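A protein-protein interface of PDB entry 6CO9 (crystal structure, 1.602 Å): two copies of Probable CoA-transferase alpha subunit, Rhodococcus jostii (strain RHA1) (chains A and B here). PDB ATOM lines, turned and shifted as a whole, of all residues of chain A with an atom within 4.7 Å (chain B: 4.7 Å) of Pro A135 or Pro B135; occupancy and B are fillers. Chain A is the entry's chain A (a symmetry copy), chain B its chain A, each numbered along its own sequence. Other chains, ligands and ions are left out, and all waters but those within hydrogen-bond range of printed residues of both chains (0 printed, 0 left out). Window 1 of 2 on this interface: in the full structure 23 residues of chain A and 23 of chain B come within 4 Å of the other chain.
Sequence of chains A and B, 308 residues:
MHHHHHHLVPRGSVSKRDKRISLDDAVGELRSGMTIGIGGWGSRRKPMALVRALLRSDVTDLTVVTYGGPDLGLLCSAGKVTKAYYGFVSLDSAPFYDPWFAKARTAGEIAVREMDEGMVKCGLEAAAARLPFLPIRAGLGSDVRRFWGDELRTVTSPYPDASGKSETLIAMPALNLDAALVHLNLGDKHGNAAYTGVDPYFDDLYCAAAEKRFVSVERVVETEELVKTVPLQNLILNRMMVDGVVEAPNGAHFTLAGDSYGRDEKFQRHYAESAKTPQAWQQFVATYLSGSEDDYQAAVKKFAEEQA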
ATOM      1  N   CYS A 122      20.237 -35.687  23.182  1.00  0.00           N
ATOM      2  CA  CYS A 122      21.426 -34.910  22.857  1.00  0.00           C
ATOM      3  C   CYS A 122      22.258 -34.618  24.097  1.00  0.00           C
ATOM      4  O   CYS A 122      23.483 -34.814  24.102  1.00  0.00           O
ATOM      5  CB  CYS A 122      20.983 -33.621  22.176  1.00  0.00           C
ATOM      6  SG  CYS A 122      22.304 -32.578  21.640  1.00  0.00           S
ATOM      7  N   LEU A 131      31.670 -34.161  26.627  1.00  0.00           N
ATOM      8  CA  LEU A 131      31.669 -32.873  25.956  1.00  0.00           C
ATOM      9  C   LEU A 131      30.816 -31.878  26.729  1.00  0.00           C
ATOM     10  O   LEU A 131      29.849 -32.269  27.394  1.00  0.00           O
ATOM     11  CB  LEU A 131      31.126 -33.002  24.531  1.00  0.00           C
ATOM     12  CG  LEU A 131      31.964 -33.846  23.561  1.00  0.00           C
ATOM     13  CD1 LEU A 131      31.163 -34.174  22.320  1.00  0.00           C
ATOM     14  CD2 LEU A 131      33.262 -33.141  23.168  1.00  0.00           C
ATOM     15  N   PHE A 133      28.869 -29.554  25.420  1.00  0.00           N
ATOM     16  CA  PHE A 133      27.624 -29.301  24.709  1.00  0.00           C
ATOM     17  C   PHE A 133      27.623 -30.117  23.430  1.00  0.00           C
ATOM     18  O   PHE A 133      28.671 -30.576  22.969  1.00  0.00           O
ATOM     19  CB  PHE A 133      27.471 -27.816  24.350  1.00  0.00           C
ATOM     20  CG  PHE A 133      28.345 -27.396  23.181  1.00  0.00           C
ATOM     21  CD1 PHE A 133      29.675 -27.048  23.380  1.00  0.00           C
ATOM     22  CD2 PHE A 133      27.842 -27.378  21.885  1.00  0.00           C
ATOM     23  CE1 PHE A 133      30.487 -26.686  22.318  1.00  0.00           C
ATOM     24  CE2 PHE A 133      28.663 -27.026  20.803  1.00  0.00           C
ATOM     25  CZ  PHE A 133      29.982 -26.668  21.031  1.00  0.00           C
ATOM     26  N   LEU A 134      26.435 -30.252  22.840  1.00  0.00           N
ATOM     27  CA  LEU A 134      26.294 -30.645  21.441  1.00  0.00           C
ATOM     28  C   LEU A 134      25.293 -29.709  20.776  1.00  0.00           C
ATOM     29  O   LEU A 134      24.317 -29.292  21.415  1.00  0.00           O
ATOM     30  CB  LEU A 134      25.813 -32.098  21.291  1.00  0.00           C
ATOM     31  CG  LEU A 134      26.835 -33.202  21.563  1.00  0.00           C
ATOM     32  CD1 LEU A 134      26.138 -34.548  21.610  1.00  0.00           C
ATOM     33  CD2 LEU A 134      27.942 -33.192  20.478  1.00  0.00           C
ATOM     34  N   PRO A 135      25.513 -29.343  19.519  1.00  0.00           N
ATOM     35  CA  PRO A 135      24.568 -28.458  18.836  1.00  0.00           C
ATOM     36  C   PRO A 135      23.344 -29.226  18.374  1.00  0.00           C
ATOM     37  O   PRO A 135      23.416 -30.406  18.016  1.00  0.00           O
ATOM     38  CB  PRO A 135      25.372 -27.954  17.635  1.00  0.00           C
ATOM     39  CG  PRO A 135      26.270 -29.133  17.314  1.00  0.00           C
ATOM     40  CD  PRO A 135      26.663 -29.693  18.663  1.00  0.00           C
ATOM     41  N   ILE A 136      22.208 -28.528  18.359  1.00  0.00           N
ATOM     42  CA  ILE A 136      20.953 -29.147  17.944  1.00  0.00           C
ATOM     43  C   ILE A 136      20.024 -28.045  17.464  1.00  0.00           C
ATOM     44  O   ILE A 136      20.086 -26.908  17.941  1.00  0.00           O
ATOM     45  CB  ILE A 136      20.325 -29.985  19.087  1.00  0.00           C
ATOM     46  CG1 ILE A 136      19.159 -30.840  18.577  1.00  0.00           C
ATOM     47  CG2 ILE A 136      19.860 -29.096  20.245  1.00  0.00           C
ATOM     48  CD1 ILE A 136      18.704 -31.928  19.563  1.00  0.00           C
ATOM     49  N   ARG A 137      19.182 -28.377  16.484  1.00  0.00           N
ATOM     50  CA  ARG A 137      18.185 -27.433  15.987  1.00  0.00           C
ATOM     51  C   ARG A 137      17.003 -27.317  16.948  1.00  0.00           C
ATOM     52  O   ARG A 137      16.546 -26.203  17.247  1.00  0.00           O
ATOM     53  CB  ARG A 137      17.721 -27.889  14.600  1.00  0.00           C
ATOM     54  CG  ARG A 137      16.942 -26.868  13.826  1.00  0.00           C
ATOM     55  CD  ARG A 137      16.685 -27.344  12.394  1.00  0.00           C
ATOM     56  NE  ARG A 137      17.709 -28.291  11.955  1.00  0.00           N
ATOM     57  CZ  ARG A 137      18.737 -27.951  11.197  1.00  0.00           C
ATOM     58  NH1 ARG A 137      18.879 -26.681  10.836  1.00  0.00           N
ATOM     59  NH2 ARG A 137      19.636 -28.865  10.842  1.00  0.00           N
ATOM     60  N   VAL A 155      25.112 -21.562  19.947  1.00  0.00           N
ATOM     61  CA  VAL A 155      26.465 -21.677  19.421  1.00  0.00           C
ATOM     62  C   VAL A 155      26.396 -21.463  17.914  1.00  0.00           C
ATOM     63  O   VAL A 155      25.516 -22.013  17.240  1.00  0.00           O
ATOM     64  CB  VAL A 155      27.102 -23.040  19.765  1.00  0.00           C
ATOM     65  CG1 VAL A 155      26.248 -24.202  19.226  1.00  0.00           C
ATOM     66  CG2 VAL A 155      28.513 -23.118  19.182  1.00  0.00           C
ATOM     67  N   LEU A 169      22.791 -22.370  16.428  1.00  0.00           N
ATOM     68  CA  LEU A 169      22.036 -23.516  16.901  1.00  0.00           C
ATOM     69  C   LEU A 169      21.946 -23.483  18.415  1.00  0.00           C
ATOM     70  O   LEU A 169      22.688 -22.759  19.081  1.00  0.00           O
ATOM     71  CB  LEU A 169      22.701 -24.820  16.469  1.00  0.00           C
ATOM     72  CG  LEU A 169      22.786 -24.970  14.961  1.00  0.00           C
ATOM     73  CD1 LEU A 169      23.999 -25.807  14.561  1.00  0.00           C
ATOM     74  CD2 LEU A 169      21.501 -25.583  14.489  1.00  0.00           C
ATOM     75  N   ILE A 170      21.028 -24.279  18.959  1.00  0.00           N
ATOM     76  CA  ILE A 170      21.030 -24.499  20.399  1.00  0.00           C
ATOM     77  C   ILE A 170      22.299 -25.244  20.775  1.00  0.00           C
ATOM     78  O   ILE A 170      22.672 -26.230  20.122  1.00  0.00           O
ATOM     79  CB  ILE A 170      19.785 -25.287  20.841  1.00  0.00           C
ATOM     80  CG1 ILE A 170      18.500 -24.536  20.473  1.00  0.00           C
ATOM     81  CG2 ILE A 170      19.846 -25.594  22.348  1.00  0.00           C
ATOM     82  CD1 ILE A 170      18.255 -23.274  21.298  1.00  0.00           C
ATOM     83  N   ALA A 171      22.987 -24.764  21.809  1.00  0.00           N
ATOM     84  CA  ALA A 171      24.089 -25.507  22.418  1.00  0.00           C
ATOM     85  C   ALA A 171      23.497 -26.285  23.578  1.00  0.00           C
ATOM     86  O   ALA A 171      23.336 -25.756  24.679  1.00  0.00           O
ATOM     87  CB  ALA A 171      25.192 -24.571  22.890  1.00  0.00           C
ATOM     88  N   CYS B 122      32.019 -38.823  13.212  1.00  0.00           N
ATOM     89  CA  CYS B 122      31.458 -37.546  13.633  1.00  0.00           C
ATOM     90  C   CYS B 122      30.963 -36.735  12.444  1.00  0.00           C
ATOM     91  O   CYS B 122      29.837 -36.214  12.454  1.00  0.00           O
ATOM     92  CB  CYS B 122      32.527 -36.787  14.409  1.00  0.00           C
ATOM     93  SG  CYS B 122      31.999 -35.233  15.065  1.00  0.00           S
ATOM     94  N   LEU B 131      23.475 -30.893  10.207  1.00  0.00           N
ATOM     95  CA  LEU B 131      24.177 -29.887  10.985  1.00  0.00           C
ATOM     96  C   LEU B 131      25.460 -29.476  10.277  1.00  0.00           C
ATOM     97  O   LEU B 131      26.061 -30.282   9.557  1.00  0.00           O
ATOM     98  CB  LEU B 131      24.519 -30.418  12.379  1.00  0.00           C
ATOM     99  CG  LEU B 131      23.327 -30.729  13.295  1.00  0.00           C
ATOM    100  CD1 LEU B 131      23.777 -31.552  14.483  1.00  0.00           C
ATOM    101  CD2 LEU B 131      22.634 -29.457  13.781  1.00  0.00           C
ATOM    102  N   PHE B 133      28.338 -28.754  11.729  1.00  0.00           N
ATOM    103  CA  PHE B 133      29.493 -29.300  12.426  1.00  0.00           C
ATOM    104  C   PHE B 133      29.005 -30.083  13.631  1.00  0.00           C
ATOM    105  O   PHE B 133      27.868 -29.916  14.078  1.00  0.00           O
ATOM    106  CB  PHE B 133      30.438 -28.190  12.905  1.00  0.00           C
ATOM    107  CG  PHE B 133      29.918 -27.455  14.128  1.00  0.00           C
ATOM    108  CD1 PHE B 133      29.014 -26.409  13.994  1.00  0.00           C
ATOM    109  CD2 PHE B 133      30.311 -27.831  15.407  1.00  0.00           C
ATOM    110  CE1 PHE B 133      28.514 -25.747  15.104  1.00  0.00           C
ATOM    111  CE2 PHE B 133      29.798 -27.174  16.536  1.00  0.00           C
ATOM    112  CZ  PHE B 133      28.910 -26.124  16.374  1.00  0.00           C
ATOM    113  N   LEU B 134      29.900 -30.907  14.175  1.00  0.00           N
ATOM    114  CA  LEU B 134      29.762 -31.429  15.532  1.00  0.00           C
ATOM    115  C   LEU B 134      31.096 -31.271  16.248  1.00  0.00           C
ATOM    116  O   LEU B 134      32.156 -31.417  15.621  1.00  0.00           O
ATOM    117  CB  LEU B 134      29.346 -32.910  15.545  1.00  0.00           C
ATOM    118  CG  LEU B 134      27.890 -33.228  15.207  1.00  0.00           C
ATOM    119  CD1 LEU B 134      27.718 -34.725  15.028  1.00  0.00           C
ATOM    120  CD2 LEU B 134      26.949 -32.695  16.318  1.00  0.00           C
ATOM    121  N   PRO B 135      31.086 -30.954  17.537  1.00  0.00           N
ATOM    122  CA  PRO B 135      32.346 -30.808  18.268  1.00  0.00           C
ATOM    123  C   PRO B 135      32.921 -32.164  18.631  1.00  0.00           C
ATOM    124  O   PRO B 135      32.193 -33.128  18.889  1.00  0.00           O
ATOM    125  CB  PRO B 135      31.929 -30.045  19.528  1.00  0.00           C
ATOM    126  CG  PRO B 135      30.518 -30.545  19.771  1.00  0.00           C
ATOM    127  CD  PRO B 135      29.914 -30.674  18.389  1.00  0.00           C
ATOM    128  N   ILE B 136      34.252 -32.223  18.675  1.00  0.00           N
ATOM    129  CA  ILE B 136      34.937 -33.469  19.004  1.00  0.00           C
ATOM    130  C   ILE B 136      36.310 -33.117  19.551  1.00  0.00           C
ATOM    131  O   ILE B 136      36.905 -32.104  19.174  1.00  0.00           O
ATOM    132  CB  ILE B 136      35.020 -34.414  17.777  1.00  0.00           C
ATOM    133  CG1 ILE B 136      35.497 -35.813  18.183  1.00  0.00           C
ATOM    134  CG2 ILE B 136      35.932 -33.841  16.688  1.00  0.00           C
ATOM    135  CD1 ILE B 136      35.293 -36.881  17.096  1.00  0.00           C
ATOM    136  N   ARG B 137      36.797 -33.945  20.478  1.00  0.00           N
ATOM    137  CA  ARG B 137      38.139 -33.764  21.027  1.00  0.00           C
ATOM    138  C   ARG B 137      39.209 -34.245  20.048  1.00  0.00           C
ATOM    139  O   ARG B 137      40.217 -33.556  19.834  1.00  0.00           O
ATOM    140  CB  ARG B 137      38.233 -34.516  22.357  1.00  0.00           C
ATOM    141  CG  ARG B 137      39.429 -34.175  23.195  1.00  0.00           C
ATOM    142  CD  ARG B 137      39.339 -34.832  24.574  1.00  0.00           C
ATOM    143  NE  ARG B 137      37.950 -35.080  24.957  1.00  0.00           N
ATOM    144  CZ  ARG B 137      37.268 -34.291  25.768  1.00  0.00           C
ATOM    145  NH1 ARG B 137      37.848 -33.193  26.239  1.00  0.00           N
ATOM    146  NH2 ARG B 137      36.002 -34.574  26.068  1.00  0.00           N
ATOM    147  N   VAL B 155      35.770 -24.716  17.762  1.00  0.00           N
ATOM    148  CA  VAL B 155      34.570 -24.101  18.311  1.00  0.00           C
ATOM    149  C   VAL B 155      34.707 -24.091  19.828  1.00  0.00           C
ATOM    150  O   VAL B 155      35.112 -25.094  20.430  1.00  0.00           O
ATOM    151  CB  VAL B 155      33.290 -24.842  17.869  1.00  0.00           C
ATOM    152  CG1 VAL B 155      33.336 -26.324  18.285  1.00  0.00           C
ATOM    153  CG2 VAL B 155      32.060 -24.169  18.479  1.00  0.00           C
ATOM    154  N   LEU B 169      37.153 -26.977  21.137  1.00  0.00           N
ATOM    155  CA  LEU B 169      37.153 -28.304  20.549  1.00  0.00           C
ATOM    156  C   LEU B 169      37.285 -28.198  19.042  1.00  0.00           C
ATOM    157  O   LEU B 169      37.090 -27.130  18.459  1.00  0.00           O
ATOM    158  CB  LEU B 169      35.862 -29.047  20.886  1.00  0.00           C
ATOM    159  CG  LEU B 169      35.669 -29.251  22.378  1.00  0.00           C
ATOM    160  CD1 LEU B 169      34.185 -29.300  22.736  1.00  0.00           C
ATOM    161  CD2 LEU B 169      36.381 -30.514  22.762  1.00  0.00           C
ATOM    162  N   ILE B 170      37.616 -29.321  18.409  1.00  0.00           N
ATOM    163  CA  ILE B 170      37.529 -29.379  16.955  1.00  0.00           C
ATOM    164  C   ILE B 170      36.071 -29.254  16.551  1.00  0.00           C
ATOM    165  O   ILE B 170      35.194 -29.916  17.126  1.00  0.00           O
ATOM    166  CB  ILE B 170      38.134 -30.687  16.415  1.00  0.00           C
ATOM    167  CG1 ILE B 170      39.610 -30.815  16.813  1.00  0.00           C
ATOM    168  CG2 ILE B 170      37.952 -30.778  14.890  1.00  0.00           C
ATOM    169  CD1 ILE B 170      40.538 -29.839  16.092  1.00  0.00           C
ATOM    170  N   ALA B 171      35.795 -28.387  15.579  1.00  0.00           N
ATOM    171  CA  ALA B 171      34.482 -28.334  14.938  1.00  0.00           C
ATOM    172  C   ALA B 171      34.569 -29.208  13.701  1.00  0.00           C
ATOM    173  O   ALA B 171      35.027 -28.768  12.645  1.00  0.00           O
ATOM    174  CB  ALA B 171      34.102 -26.906  14.576  1.00  0.00           C
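Hydrophobic or aromatic side chains of chain B that line the printed part of chain A: Leu B131, Leu B134, Pro B135, Val B155 and Leu B169.
Of the 11 printed residues of chain A, 6 touch a printed residue of chain B.
Hydrophobic or aromatic side chains of chain A that line the printed part of chain B: Leu A131, Leu A134, Pro A135, Val A155 and Leu A169.
Among the printed residues, no Asp or Glu carboxylate lies within 4 Å of a Lys or Arg side-chain nitrogen of the other chain.
Printed residues of chain B within 4 Å of Leu A134: Pro B135 (3.8 Å).
Pro A135 touches just these residues of chain B: Leu B131 (3.7 Å), Phe B133 (3.7 Å), Leu B134 (3.8 Å) and Pro B135 (3.4 Å).
Arg A137 touches none of the printed residues of chain B.
Of the printed residues of chain B, Leu A169 touches Leu B131 (3.97 Å).
Printed residues of chain A within 4 Å of Phe B133: Pro A135 (3.7 Å).
Of the printed residues of chain A, Val B155 touches Val A155.
The nearest printed residue of chain A that does not touch Val B155 is Phe A133 (4.1 Å).
O of Pro B135 touches CD1 of Leu A131 (3.7 Å).
Leu A131 touches Leu B169.
Pro B135 touches Phe A133 (CG to O, 3.7 Å).
Leu A134 touches Pro B135.
Pro A135 touches Leu B131.
Pro A135 touches Phe B133 (CG to O, 3.7 Å).
Pro A135 touches Leu B134 (CG to CD2, 3.8 Å).
Pro A135 touches Pro B135 (CD to CD, 3.4 Å).
CG2 of Val A155 touches CG2 of Val B155 (3.8 Å).
Leu A169 touches Leu B131 (CD1 to CD2, 3.97 Å).
Leu A131 touches Pro B135, and with the chains exchanged Pro A135 touches Leu B131.
Phe A133 touches Pro B135, and with the chains exchanged Pro A135 touches Phe B133.
Pro B135 touches its own counterpart, Pro A135.
Val B155 touches its own counterpart, Val A155.
Of the 10 pairs that touch across the chains among the printed residues, 10 have their exchanged pair printed and touching as well.
N of Val B155 lies within hydrogen-bond range of O of Leu B169, 2.8 Å away.
The backbone NH (N) of Val A155 sits at hydrogen-bond distance from the backbone carbonyl oxygen (O) of Leu A169 (2.8 Å).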
